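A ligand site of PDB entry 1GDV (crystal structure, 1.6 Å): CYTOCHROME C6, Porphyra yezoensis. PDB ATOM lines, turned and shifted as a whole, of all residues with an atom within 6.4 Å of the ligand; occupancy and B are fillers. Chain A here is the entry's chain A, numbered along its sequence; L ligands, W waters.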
ATOM      1  N   VAL A   9       7.944  -0.936  -0.142  1.00  0.00           N
ATOM      2  CA  VAL A   9       6.738  -1.448   0.517  1.00  0.00           C
ATOM      3  C   VAL A   9       5.821  -2.025  -0.550  1.00  0.00           C
ATOM      4  O   VAL A   9       5.250  -3.108  -0.351  1.00  0.00           O
ATOM      5  CB  VAL A   9       6.002  -0.310   1.278  1.00  0.00           C
ATOM      6  CG1 VAL A   9       4.607  -0.764   1.701  1.00  0.00           C
ATOM      7  CG2 VAL A   9       6.813   0.078   2.495  1.00  0.00           C
ATOM      8  N   PHE A  10       5.697  -1.302  -1.662  1.00  0.00           N
ATOM      9  CA  PHE A  10       4.842  -1.716  -2.775  1.00  0.00           C
ATOM     10  C   PHE A  10       5.315  -3.049  -3.335  1.00  0.00           C
ATOM     11  O   PHE A  10       4.515  -3.966  -3.577  1.00  0.00           O
ATOM     12  CB  PHE A  10       4.855  -0.673  -3.886  1.00  0.00           C
ATOM     13  CG  PHE A  10       3.868  -0.959  -4.985  1.00  0.00           C
ATOM     14  CD1 PHE A  10       2.550  -0.537  -4.871  1.00  0.00           C
ATOM     15  CD2 PHE A  10       4.250  -1.657  -6.116  1.00  0.00           C
ATOM     16  CE1 PHE A  10       1.622  -0.831  -5.875  1.00  0.00           C
ATOM     17  CE2 PHE A  10       3.329  -1.944  -7.121  1.00  0.00           C
ATOM     18  CZ  PHE A  10       2.019  -1.527  -6.990  1.00  0.00           C
ATOM     19  N   ASN A  13       4.737  -5.859  -0.802  1.00  0.00           N
ATOM     20  CA  ASN A  13       3.369  -6.067  -0.344  1.00  0.00           C
ATOM     21  C   ASN A  13       2.246  -5.971  -1.341  1.00  0.00           C
ATOM     22  O   ASN A  13       1.148  -6.493  -1.086  1.00  0.00           O
ATOM     23  CB  ASN A  13       3.043  -5.089   0.774  1.00  0.00           C
ATOM     24  CG  ASN A  13       3.920  -5.259   1.983  1.00  0.00           C
ATOM     25  OD1 ASN A  13       3.577  -6.031   2.874  1.00  0.00           O
ATOM     26  ND2 ASN A  13       5.046  -4.543   2.034  1.00  0.00           N
ATOM     27  N   CYS A  14       2.501  -5.278  -2.448  1.00  0.00           N
ATOM     28  CA  CYS A  14       1.459  -4.996  -3.427  1.00  0.00           C
ATOM     29  C   CYS A  14       1.622  -5.575  -4.811  1.00  0.00           C
ATOM     30  O   CYS A  14       0.638  -5.740  -5.542  1.00  0.00           O
ATOM     31  CB  CYS A  14       1.290  -3.479  -3.589  1.00  0.00           C
ATOM     32  SG  CYS A  14       1.330  -2.533  -2.041  1.00  0.00           S
ATOM     33  N   ALA A  15       2.864  -5.840  -5.179  1.00  0.00           N
ATOM     34  CA  ALA A  15       3.167  -6.345  -6.510  1.00  0.00           C
ATOM     35  C   ALA A  15       2.541  -7.719  -6.787  1.00  0.00           C
ATOM     36  O   ALA A  15       2.316  -8.067  -7.955  1.00  0.00           O
ATOM     37  CB  ALA A  15       4.691  -6.399  -6.699  1.00  0.00           C
ATOM     38  N   ALA A  16       2.246  -8.479  -5.734  1.00  0.00           N
ATOM     39  CA  ALA A  16       1.608  -9.786  -5.899  1.00  0.00           C
ATOM     40  C   ALA A  16       0.290  -9.638  -6.690  1.00  0.00           C
ATOM     41  O   ALA A  16      -0.111 -10.546  -7.413  1.00  0.00           O
ATOM     42  CB  ALA A  16       1.339 -10.416  -4.544  1.00  0.00           C
ATOM     43  N   CYS A  17      -0.368  -8.481  -6.573  1.00  0.00           N
ATOM     44  CA  CYS A  17      -1.620  -8.285  -7.293  1.00  0.00           C
ATOM     45  C   CYS A  17      -1.699  -7.063  -8.181  1.00  0.00           C
ATOM     46  O   CYS A  17      -2.607  -6.964  -9.008  1.00  0.00           O
ATOM     47  CB  CYS A  17      -2.795  -8.233  -6.318  1.00  0.00           C
ATOM     48  SG  CYS A  17      -2.922  -9.652  -5.189  1.00  0.00           S
ATOM     49  N   HIS A  18      -0.768  -6.122  -8.006  1.00  0.00           N
ATOM     50  CA  HIS A  18      -0.799  -4.868  -8.762  1.00  0.00           C
ATOM     51  C   HIS A  18       0.484  -4.471  -9.486  1.00  0.00           C
ATOM     52  O   HIS A  18       0.685  -3.303  -9.794  1.00  0.00           O
ATOM     53  CB  HIS A  18      -1.161  -3.722  -7.791  1.00  0.00           C
ATOM     54  CG  HIS A  18      -2.528  -3.795  -7.140  1.00  0.00           C
ATOM     55  ND1 HIS A  18      -3.720  -3.667  -7.792  1.00  0.00           N
ATOM     56  CD2 HIS A  18      -2.665  -3.966  -5.759  1.00  0.00           C
ATOM     57  CE1 HIS A  18      -4.608  -3.686  -6.823  1.00  0.00           C
ATOM     58  NE2 HIS A  18      -4.051  -3.790  -5.650  1.00  0.00           N
ATOM     59  N   ASN A  23      -4.322  -5.154 -11.958  1.00  0.00           N
ATOM     60  CA  ASN A  23      -5.061  -5.869 -10.912  1.00  0.00           C
ATOM     61  C   ASN A  23      -5.235  -7.308 -11.429  1.00  0.00           C
ATOM     62  O   ASN A  23      -5.993  -7.576 -12.360  1.00  0.00           O
ATOM     63  CB  ASN A  23      -6.411  -5.232 -10.606  1.00  0.00           C
ATOM     64  CG  ASN A  23      -7.016  -5.814  -9.330  1.00  0.00           C
ATOM     65  OD1 ASN A  23      -7.000  -7.028  -9.158  1.00  0.00           O
ATOM     66  ND2 ASN A  23      -7.506  -4.969  -8.440  1.00  0.00           N
ATOM     67  N   ILE A  25      -6.624  -9.842 -10.179  1.00  0.00           N
ATOM     68  CA  ILE A  25      -7.861 -10.531  -9.809  1.00  0.00           C
ATOM     69  C   ILE A  25      -9.120  -9.936 -10.462  1.00  0.00           C
ATOM     70  O   ILE A  25      -9.936 -10.666 -11.025  1.00  0.00           O
ATOM     71  CB  ILE A  25      -7.995 -10.515  -8.236  1.00  0.00           C
ATOM     72  CG1 ILE A  25      -6.759 -11.177  -7.633  1.00  0.00           C
ATOM     73  CG2 ILE A  25      -9.263 -11.228  -7.765  1.00  0.00           C
ATOM     74  CD1 ILE A  25      -6.689 -11.072  -6.157  1.00  0.00           C
ATOM     75  N   MET A  26      -9.265  -8.609 -10.354  1.00  0.00           N
ATOM     76  CA  MET A  26     -10.409  -7.860 -10.922  1.00  0.00           C
ATOM     77  C   MET A  26      -9.763  -6.862 -11.844  1.00  0.00           C
ATOM     78  O   MET A  26      -9.418  -5.753 -11.408  1.00  0.00           O
ATOM     79  CB  MET A  26     -11.165  -7.090  -9.845  1.00  0.00           C
ATOM     80  CG  MET A  26     -11.721  -7.929  -8.768  1.00  0.00           C
ATOM     81  SD  MET A  26     -12.818  -6.936  -7.770  1.00  0.00           S
ATOM     82  CE  MET A  26     -13.823  -8.270  -7.055  1.00  0.00           C
ATOM     83  N   ASP A  28     -10.616  -4.670 -13.761  1.00  0.00           N
ATOM     84  CA  ASP A  28     -11.135  -3.318 -13.843  1.00  0.00           C
ATOM     85  C   ASP A  28     -10.690  -2.385 -12.716  1.00  0.00           C
ATOM     86  O   ASP A  28     -10.791  -1.155 -12.833  1.00  0.00           O
ATOM     87  CB  ASP A  28     -12.664  -3.370 -13.847  1.00  0.00           C
ATOM     88  CG  ASP A  28     -13.224  -3.975 -12.564  1.00  0.00           C
ATOM     89  OD1 ASP A  28     -14.237  -3.457 -12.039  1.00  0.00           O
ATOM     90  OD2 ASP A  28     -12.640  -4.975 -12.076  1.00  0.00           O
ATOM     91  N   LYS A  29     -10.209  -2.950 -11.620  1.00  0.00           N
ATOM     92  CA  LYS A  29      -9.808  -2.125 -10.498  1.00  0.00           C
ATOM     93  C   LYS A  29      -8.299  -1.923 -10.482  1.00  0.00           C
ATOM     94  O   LYS A  29      -7.617  -2.270  -9.507  1.00  0.00           O
ATOM     95  CB  LYS A  29     -10.294  -2.767  -9.214  1.00  0.00           C
ATOM     96  CG  LYS A  29     -11.782  -2.999  -9.225  1.00  0.00           C
ATOM     97  CD  LYS A  29     -12.475  -1.685  -9.302  1.00  0.00           C
ATOM     98  CE  LYS A  29     -13.119  -1.382  -7.984  1.00  0.00           C
ATOM     99  NZ  LYS A  29     -14.510  -1.926  -8.027  1.00  0.00           N
ATOM    100  N   THR A  30      -7.786  -1.336 -11.544  1.00  0.00           N
ATOM    101  CA  THR A  30      -6.356  -1.123 -11.635  1.00  0.00           C
ATOM    102  C   THR A  30      -5.899   0.135 -10.910  1.00  0.00           C
ATOM    103  O   THR A  30      -6.698   0.828 -10.296  1.00  0.00           O
ATOM    104  CB  THR A  30      -5.966  -1.032 -13.077  1.00  0.00           C
ATOM    105  OG1 THR A  30      -6.587   0.146 -13.640  1.00  0.00           O
ATOM    106  CG2 THR A  30      -6.427  -2.301 -13.814  1.00  0.00           C
ATOM    107  N   LEU A  31      -4.604   0.397 -10.993  1.00  0.00           N
ATOM    108  CA  LEU A  31      -4.016   1.560 -10.330  1.00  0.00           C
ATOM    109  C   LEU A  31      -3.689   2.682 -11.344  1.00  0.00           C
ATOM    110  O   LEU A  31      -2.872   3.563 -11.073  1.00  0.00           O
ATOM    111  CB  LEU A  31      -2.743   1.126  -9.588  1.00  0.00           C
ATOM    112  CG  LEU A  31      -2.844   0.575  -8.168  1.00  0.00           C
ATOM    113  CD1 LEU A  31      -4.187  -0.119  -7.896  1.00  0.00           C
ATOM    114  CD2 LEU A  31      -1.667  -0.316  -7.911  1.00  0.00           C
ATOM    115  N   LYS A  32      -4.335   2.625 -12.513  1.00  0.00           N
ATOM    116  CA  LYS A  32      -4.139   3.613 -13.577  1.00  0.00           C
ATOM    117  C   LYS A  32      -4.896   4.913 -13.242  1.00  0.00           C
ATOM    118  O   LYS A  32      -6.025   4.867 -12.732  1.00  0.00           O
ATOM    119  CB  LYS A  32      -4.661   3.042 -14.907  1.00  0.00           C
ATOM    120  CG  LYS A  32      -3.907   1.824 -15.402  1.00  0.00           C
ATOM    121  CD  LYS A  32      -2.421   2.109 -15.400  1.00  0.00           C
ATOM    122  CE  LYS A  32      -1.607   0.837 -15.494  1.00  0.00           C
ATOM    123  NZ  LYS A  32      -0.841   0.876 -16.752  1.00  0.00           N
ATOM    124  N   VAL A  35      -8.709   5.312 -13.881  1.00  0.00           N
ATOM    125  CA  VAL A  35      -9.548   4.415 -13.104  1.00  0.00           C
ATOM    126  C   VAL A  35      -9.556   4.871 -11.664  1.00  0.00           C
ATOM    127  O   VAL A  35     -10.595   4.853 -10.997  1.00  0.00           O
ATOM    128  CB  VAL A  35      -9.031   2.960 -13.193  1.00  0.00           C
ATOM    129  CG1 VAL A  35      -9.860   2.017 -12.318  1.00  0.00           C
ATOM    130  CG2 VAL A  35      -9.076   2.518 -14.661  1.00  0.00           C
ATOM    131  N   LEU A  36      -8.409   5.294 -11.185  1.00  0.00           N
ATOM    132  CA  LEU A  36      -8.312   5.793  -9.830  1.00  0.00           C
ATOM    133  C   LEU A  36      -9.241   7.019  -9.727  1.00  0.00           C
ATOM    134  O   LEU A  36      -9.997   7.127  -8.743  1.00  0.00           O
ATOM    135  CB  LEU A  36      -6.869   6.153  -9.506  1.00  0.00           C
ATOM    136  CG  LEU A  36      -6.006   5.247  -8.594  1.00  0.00           C
ATOM    137  CD1 LEU A  36      -6.557   3.865  -8.513  1.00  0.00           C
ATOM    138  CD2 LEU A  36      -4.579   5.242  -9.077  1.00  0.00           C
ATOM    139  N   ASN A  39     -12.919   5.990  -9.645  1.00  0.00           N
ATOM    140  CA  ASN A  39     -13.325   5.353  -8.409  1.00  0.00           C
ATOM    141  C   ASN A  39     -13.088   6.191  -7.161  1.00  0.00           C
ATOM    142  O   ASN A  39     -13.136   5.652  -6.058  1.00  0.00           O
ATOM    143  CB  ASN A  39     -12.557   4.044  -8.230  1.00  0.00           C
ATOM    144  CG  ASN A  39     -13.069   2.965  -9.123  1.00  0.00           C
ATOM    145  OD1 ASN A  39     -14.274   2.857  -9.339  1.00  0.00           O
ATOM    146  ND2 ASN A  39     -12.161   2.138  -9.663  1.00  0.00           N
ATOM    147  N   MET A  41     -10.441   7.261  -5.897  1.00  0.00           N
ATOM    148  CA  MET A  41      -9.328   6.686  -5.147  1.00  0.00           C
ATOM    149  C   MET A  41      -8.044   7.416  -5.507  1.00  0.00           C
ATOM    150  O   MET A  41      -6.943   6.833  -5.467  1.00  0.00           O
ATOM    151  CB  MET A  41      -9.166   5.190  -5.486  1.00  0.00           C
ATOM    152  CG  MET A  41     -10.311   4.310  -4.990  1.00  0.00           C
ATOM    153  SD  MET A  41     -10.366   4.201  -3.201  1.00  0.00           S
ATOM    154  CE  MET A  41      -8.744   3.963  -2.848  1.00  0.00           C
ATOM    155  N   ILE A  47      -6.809   6.233  -0.388  1.00  0.00           N
ATOM    156  CA  ILE A  47      -5.924   5.082  -0.588  1.00  0.00           C
ATOM    157  C   ILE A  47      -5.360   4.548   0.737  1.00  0.00           C
ATOM    158  O   ILE A  47      -5.347   3.344   0.958  1.00  0.00           O
ATOM    159  CB  ILE A  47      -4.764   5.441  -1.547  1.00  0.00           C
ATOM    160  CG1 ILE A  47      -5.333   5.789  -2.914  1.00  0.00           C
ATOM    161  CG2 ILE A  47      -3.779   4.274  -1.650  1.00  0.00           C
ATOM    162  CD1 ILE A  47      -4.286   6.188  -3.889  1.00  0.00           C
ATOM    163  N   GLN A  50      -8.026   2.357   2.333  1.00  0.00           N
ATOM    164  CA  GLN A  50      -8.223   1.086   1.664  1.00  0.00           C
ATOM    165  C   GLN A  50      -7.085   0.106   1.986  1.00  0.00           C
ATOM    166  O   GLN A  50      -7.319  -1.105   2.175  1.00  0.00           O
ATOM    167  CB  GLN A  50      -8.333   1.287   0.156  1.00  0.00           C
ATOM    168  CG  GLN A  50      -8.307  -0.009  -0.647  1.00  0.00           C
ATOM    169  CD  GLN A  50      -9.550  -0.186  -1.508  1.00  0.00           C
ATOM    170  OE1 GLN A  50      -9.600  -1.072  -2.380  1.00  0.00           O
ATOM    171  NE2 GLN A  50     -10.536   0.645  -1.281  1.00  0.00           N
ATOM    172  N   VAL A  51      -5.859   0.622   2.054  1.00  0.00           N
ATOM    173  CA  VAL A  51      -4.728  -0.206   2.382  1.00  0.00           C
ATOM    174  C   VAL A  51      -4.835  -0.668   3.826  1.00  0.00           C
ATOM    175  O   VAL A  51      -4.618  -1.834   4.130  1.00  0.00           O
ATOM    176  CB  VAL A  51      -3.413   0.564   2.187  1.00  0.00           C
ATOM    177  CG1 VAL A  51      -2.256  -0.219   2.775  1.00  0.00           C
ATOM    178  CG2 VAL A  51      -3.199   0.835   0.691  1.00  0.00           C
ATOM    179  N   LYS A  55     -10.279  -4.568   1.381  1.00  0.00           N
ATOM    180  CA  LYS A  55     -11.573  -4.512   0.725  1.00  0.00           C
ATOM    181  C   LYS A  55     -11.762  -5.777  -0.116  1.00  0.00           C
ATOM    182  O   LYS A  55     -11.021  -6.014  -1.079  1.00  0.00           O
ATOM    183  CB  LYS A  55     -11.666  -3.280  -0.176  1.00  0.00           C
ATOM    184  CG  LYS A  55     -13.022  -3.117  -0.821  1.00  0.00           C
ATOM    185  CD  LYS A  55     -13.555  -1.732  -0.594  1.00  0.00           C
ATOM    186  CE  LYS A  55     -14.716  -1.410  -1.530  1.00  0.00           C
ATOM    187  NZ  LYS A  55     -14.292  -0.771  -2.832  1.00  0.00           N
ATOM    188  N   ASN A  56     -12.754  -6.571   0.238  1.00  0.00           N
ATOM    189  CA  ASN A  56     -13.030  -7.822  -0.481  1.00  0.00           C
ATOM    190  C   ASN A  56     -11.783  -8.736  -0.579  1.00  0.00           C
ATOM    191  O   ASN A  56     -11.252  -9.144   0.442  1.00  0.00           O
ATOM    192  CB  ASN A  56     -13.584  -7.518  -1.877  1.00  0.00           C
ATOM    193  CG  ASN A  56     -14.385  -8.700  -2.467  1.00  0.00           C
ATOM    194  OD1 ASN A  56     -14.981  -9.489  -1.710  1.00  0.00           O
ATOM    195  ND2 ASN A  56     -14.404  -8.815  -3.811  1.00  0.00           N
ATOM    196  N   ALA A  57     -11.316  -9.057  -1.794  1.00  0.00           N
ATOM    197  CA  ALA A  57     -10.150  -9.912  -1.953  1.00  0.00           C
ATOM    198  C   ALA A  57      -8.821  -9.210  -1.662  1.00  0.00           C
ATOM    199  O   ALA A  57      -7.786  -9.844  -1.626  1.00  0.00           O
ATOM    200  CB  ALA A  57     -10.119 -10.528  -3.364  1.00  0.00           C
ATOM    201  N   MET A  58      -8.856  -7.894  -1.449  1.00  0.00           N
ATOM    202  CA  MET A  58      -7.620  -7.197  -1.105  1.00  0.00           C
ATOM    203  C   MET A  58      -7.452  -7.261   0.409  1.00  0.00           C
ATOM    204  O   MET A  58      -8.372  -6.879   1.163  1.00  0.00           O
ATOM    205  CB  MET A  58      -7.665  -5.731  -1.507  1.00  0.00           C
ATOM    206  CG  MET A  58      -6.464  -4.949  -0.977  1.00  0.00           C
ATOM    207  SD  MET A  58      -6.261  -3.396  -1.850  1.00  0.00           S
ATOM    208  CE  MET A  58      -5.268  -2.488  -0.705  1.00  0.00           C
ATOM    209  N   PRO A  59      -6.298  -7.741   0.891  1.00  0.00           N
ATOM    210  CA  PRO A  59      -6.072  -7.825   2.338  1.00  0.00           C
ATOM    211  C   PRO A  59      -5.943  -6.456   3.018  1.00  0.00           C
ATOM    212  O   PRO A  59      -5.658  -5.466   2.366  1.00  0.00           O
ATOM    213  CB  PRO A  59      -4.751  -8.607   2.474  1.00  0.00           C
ATOM    214  CG  PRO A  59      -4.108  -8.567   1.150  1.00  0.00           C
ATOM    215  CD  PRO A  59      -5.156  -8.263   0.111  1.00  0.00           C
ATOM    216  N   PHE A  61      -3.906  -4.116   5.639  1.00  0.00           N
ATOM    217  CA  PHE A  61      -2.515  -4.096   6.040  1.00  0.00           C
ATOM    218  C   PHE A  61      -2.285  -3.301   7.314  1.00  0.00           C
ATOM    219  O   PHE A  61      -1.142  -3.144   7.753  1.00  0.00           O
ATOM    220  CB  PHE A  61      -1.646  -3.502   4.925  1.00  0.00           C
ATOM    221  CG  PHE A  61      -1.579  -4.348   3.679  1.00  0.00           C
ATOM    222  CD1 PHE A  61      -2.600  -4.291   2.726  1.00  0.00           C
ATOM    223  CD2 PHE A  61      -0.498  -5.194   3.450  1.00  0.00           C
ATOM    224  CE1 PHE A  61      -2.534  -5.057   1.569  1.00  0.00           C
ATOM    225  CE2 PHE A  61      -0.438  -5.966   2.294  1.00  0.00           C
ATOM    226  CZ  PHE A  61      -1.480  -5.891   1.354  1.00  0.00           C
ATOM    227  N   LEU A  65       1.512  -3.387   8.343  1.00  0.00           N
ATOM    228  CA  LEU A  65       2.371  -2.287   7.956  1.00  0.00           C
ATOM    229  C   LEU A  65       2.266  -1.122   8.935  1.00  0.00           C
ATOM    230  O   LEU A  65       1.156  -0.745   9.382  1.00  0.00           O
ATOM    231  CB  LEU A  65       2.039  -1.804   6.544  1.00  0.00           C
ATOM    232  CG  LEU A  65       3.005  -2.230   5.429  1.00  0.00           C
ATOM    233  CD1 LEU A  65       3.548  -3.620   5.729  1.00  0.00           C
ATOM    234  CD2 LEU A  65       2.288  -2.188   4.091  1.00  0.00           C
ATOM    235  N   ALA A  73       3.589   4.183   0.636  1.00  0.00           N
ATOM    236  CA  ALA A  73       3.078   3.324  -0.442  1.00  0.00           C
ATOM    237  C   ALA A  73       1.957   4.068  -1.170  1.00  0.00           C
ATOM    238  O   ALA A  73       1.925   4.059  -2.414  1.00  0.00           O
ATOM    239  CB  ALA A  73       2.581   1.969   0.096  1.00  0.00           C
ATOM    240  N   ALA A  74       1.070   4.738  -0.429  1.00  0.00           N
ATOM    241  CA  ALA A  74      -0.029   5.479  -1.055  1.00  0.00           C
ATOM    242  C   ALA A  74       0.530   6.520  -2.005  1.00  0.00           C
ATOM    243  O   ALA A  74       0.047   6.703  -3.114  1.00  0.00           O
ATOM    244  CB  ALA A  74      -0.903   6.174   0.003  1.00  0.00           C
ATOM    245  N   VAL A  77       2.020   4.985  -5.188  1.00  0.00           N
ATOM    246  CA  VAL A  77       0.967   4.633  -6.136  1.00  0.00           C
ATOM    247  C   VAL A  77       0.472   5.858  -6.895  1.00  0.00           C
ATOM    248  O   VAL A  77       0.220   5.804  -8.102  1.00  0.00           O
ATOM    249  CB  VAL A  77      -0.223   3.986  -5.404  1.00  0.00           C
ATOM    250  CG1 VAL A  77      -1.413   3.886  -6.338  1.00  0.00           C
ATOM    251  CG2 VAL A  77       0.203   2.591  -4.846  1.00  0.00           C
HETATM  252 FE1  LIG L   1      -5.072  -3.648  -3.854  1.00  0.00          FE
HETATM  253  C1  LIG L   1      -8.006  -2.444  -5.131  1.00  0.00           C
HETATM  254  C2  LIG L   1      -3.866  -0.514  -3.535  1.00  0.00           C
HETATM  255  C3  LIG L   1      -2.321  -4.921  -2.236  1.00  0.00           C
HETATM  256  C4  LIG L   1      -6.093  -6.826  -4.554  1.00  0.00           C
HETATM  257  N1  LIG L   1      -5.734  -1.877  -4.310  1.00  0.00           N
HETATM  258  C5  LIG L   1      -6.952  -1.540  -4.865  1.00  0.00           C
HETATM  259  C6  LIG L   1      -7.026  -0.076  -5.107  1.00  0.00           C
HETATM  260  C7  LIG L   1      -5.895   0.432  -4.589  1.00  0.00           C
HETATM  261  C8  LIG L   1      -5.102  -0.666  -4.110  1.00  0.00           C
HETATM  262  C9  LIG L   1      -5.516   1.933  -4.504  1.00  0.00           C
HETATM  263  C10 LIG L   1      -8.219   0.673  -5.766  1.00  0.00           C
HETATM  264  C11 LIG L   1      -8.105   0.564  -7.284  1.00  0.00           C
HETATM  265  C12 LIG L   1      -9.316   1.106  -8.018  1.00  0.00           C
HETATM  266  O1  LIG L   1     -10.273   1.529  -7.373  1.00  0.00           O
HETATM  267  O2  LIG L   1      -9.305   1.113  -9.267  1.00  0.00           O
HETATM  268  N2  LIG L   1      -3.494  -2.888  -3.021  1.00  0.00           N
HETATM  269  C13 LIG L   1      -3.110  -1.552  -3.035  1.00  0.00           C
HETATM  270  C14 LIG L   1      -1.803  -1.331  -2.387  1.00  0.00           C
HETATM  271  C15 LIG L   1      -1.398  -2.562  -1.904  1.00  0.00           C
HETATM  272  C16 LIG L   1      -2.454  -3.521  -2.364  1.00  0.00           C
HETATM  273  C17 LIG L   1      -1.019  -0.016  -2.312  1.00  0.00           C
HETATM  274  C18 LIG L   1      -0.219  -2.832  -1.122  1.00  0.00           C
HETATM  275  C19 LIG L   1      -0.276  -2.295   0.315  1.00  0.00           C
HETATM  276  N3  LIG L   1      -4.391  -5.478  -3.421  1.00  0.00           N
HETATM  277  C20 LIG L   1      -3.249  -5.852  -2.749  1.00  0.00           C
HETATM  278  C21 LIG L   1      -3.016  -7.228  -2.776  1.00  0.00           C
HETATM  279  C22 LIG L   1      -4.056  -7.769  -3.515  1.00  0.00           C
HETATM  280  C23 LIG L   1      -4.895  -6.678  -3.872  1.00  0.00           C
HETATM  281  C24 LIG L   1      -1.808  -7.930  -2.158  1.00  0.00           C
HETATM  282  C25 LIG L   1      -4.229  -9.153  -4.019  1.00  0.00           C
HETATM  283  C26 LIG L   1      -4.208 -10.278  -2.990  1.00  0.00           C
HETATM  284  N4  LIG L   1      -6.726  -4.441  -4.637  1.00  0.00           N
HETATM  285  C27 LIG L   1      -6.979  -5.792  -4.858  1.00  0.00           C
HETATM  286  C28 LIG L   1      -8.340  -5.998  -5.274  1.00  0.00           C
HETATM  287  C29 LIG L   1      -8.919  -4.771  -5.381  1.00  0.00           C
HETATM  288  C30 LIG L   1      -7.890  -3.815  -4.999  1.00  0.00           C
HETATM  289  C31 LIG L   1      -8.929  -7.362  -5.622  1.00  0.00           C
HETATM  290  C32 LIG L   1     -10.362  -4.446  -5.798  1.00  0.00           C
HETATM  291  C33 LIG L   1     -11.177  -4.530  -4.505  1.00  0.00           C
HETATM  292  C34 LIG L   1     -12.660  -4.357  -4.770  1.00  0.00           C
HETATM  293  O3  LIG L   1     -13.035  -3.310  -5.335  1.00  0.00           O
HETATM  294  O4  LIG L   1     -13.437  -5.270  -4.434  1.00  0.00           O
HETATM  295  O   HOH W   1       0.585  -8.945   0.100  1.00  0.00           O
HETATM  296  O   HOH W   2     -12.850   1.457  -6.015  1.00  0.00           O
HETATM  297  O   HOH W   3     -11.481  -1.087  -4.564  1.00  0.00           O
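OD1 of Asn 23 lies within hydrogen-bond range of N of Met 26 (3.0 Å).
The backbone carbonyl oxygen (O) of Val 51 sits at hydrogen-bond distance from the backbone NH (N) of Phe 61 (2.8 Å).
The side-chain amide oxygen of Asn 23 is in hydrogen-bond range of the backbone NH of Ile 25 (3.0 Å).
The backbone carbonyl oxygen (O) of Leu 36 is in hydrogen-bond range of the backbone NH (N) of Met 41, 2.9 Å away.
The backbone carbonyl oxygen (O) of Val 9 lies within hydrogen-bond range of the side-chain amide nitrogen (ND2) of Asn 13 (2.8 Å).
O of Val 35 lies within hydrogen-bond range of ND2 of Asn 39, at 3.4 Å.
The side-chain amide nitrogen (ND2) of Asn 23 lies within hydrogen-bond range of the backbone carbonyl oxygen (O) of Lys 29.
O4 of the ligand lies close to SD of Met 26 (3.8 Å).
O of Asn 13 touches C24 of the ligand (3.5 Å).
Asn 23 touches the ligand (ND2 to C29, 3.4 Å).
Ile 25 touches the ligand.
Leu 31 touches the ligand.
CG1 of Val 35 touches O2 of the ligand, 3.2 Å away.
Leu 36 touches the ligand.
Met 41 touches the ligand.
Gln 50 touches the ligand.
Val 51 touches the ligand.
Asn 56 touches the ligand (CB to O4, 3.4 Å).
Ala 57 touches the ligand.
CD of Pro 59 touches C21 of the ligand, 3.7 Å away.
Phe 61 touches the ligand (CE1 to C19, 3.8 Å).
CG2 of Val 77 touches C17 of the ligand, 3.8 Å away.
Hydrophobic or aromatic side chains within 4 Å of the ligand: His 18, Ile 25, Met 26, Leu 31, Val 35, Leu 36, Met 41, Val 51, Met 58, Pro 59, Phe 61 and Val 77.
23 residues have an atom within 4 Å of the ligand: Asn 13, Cys 14, Cys 17, His 18, Asn 23, Ile 25, Met 26, Lys 29, Thr 30, Leu 31, Val 35, Leu 36, Asn 39, Met 41, Gln 50, Val 51, Lys 55, Asn 56, Ala 57, Met 58, Pro 59, Phe 61 and Val 77.
Water W3 lies within hydrogen-bond range of O3 of the ligand (2.8 Å), OE1 of Gln 50 (2.9 Å) and NZ of Lys 55 (3.3 Å).
NZ of Lys 29 lies within salt-bridge range of O3 of the ligand, at 3.4 Å.
SD of Met 58 binds FE1 of the ligand (2.3 Å).
NE2 of His 18 binds FE1 of the ligand (2.1 Å).
The side-chain sulfur (SG) of Cys 14 is covalently linked to a carbon (C18) of the ligand (1.8 Å).
C25 of the ligand is bonded to SG of Cys 17, at 1.8 Å.
The side-chain amide nitrogen (ND2) of Asn 39 is in hydrogen-bond range of an oxygen (O1) of the ligand (3.0 Å).
The side-chain amino group (NZ) of Lys 55 is in salt-bridge range of an oxygen (O3) of the ligand, 3.8 Å away.
The backbone carbonyl oxygen (O) of Thr 30 lies close to an oxygen (O2) of the ligand (2.8 Å).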
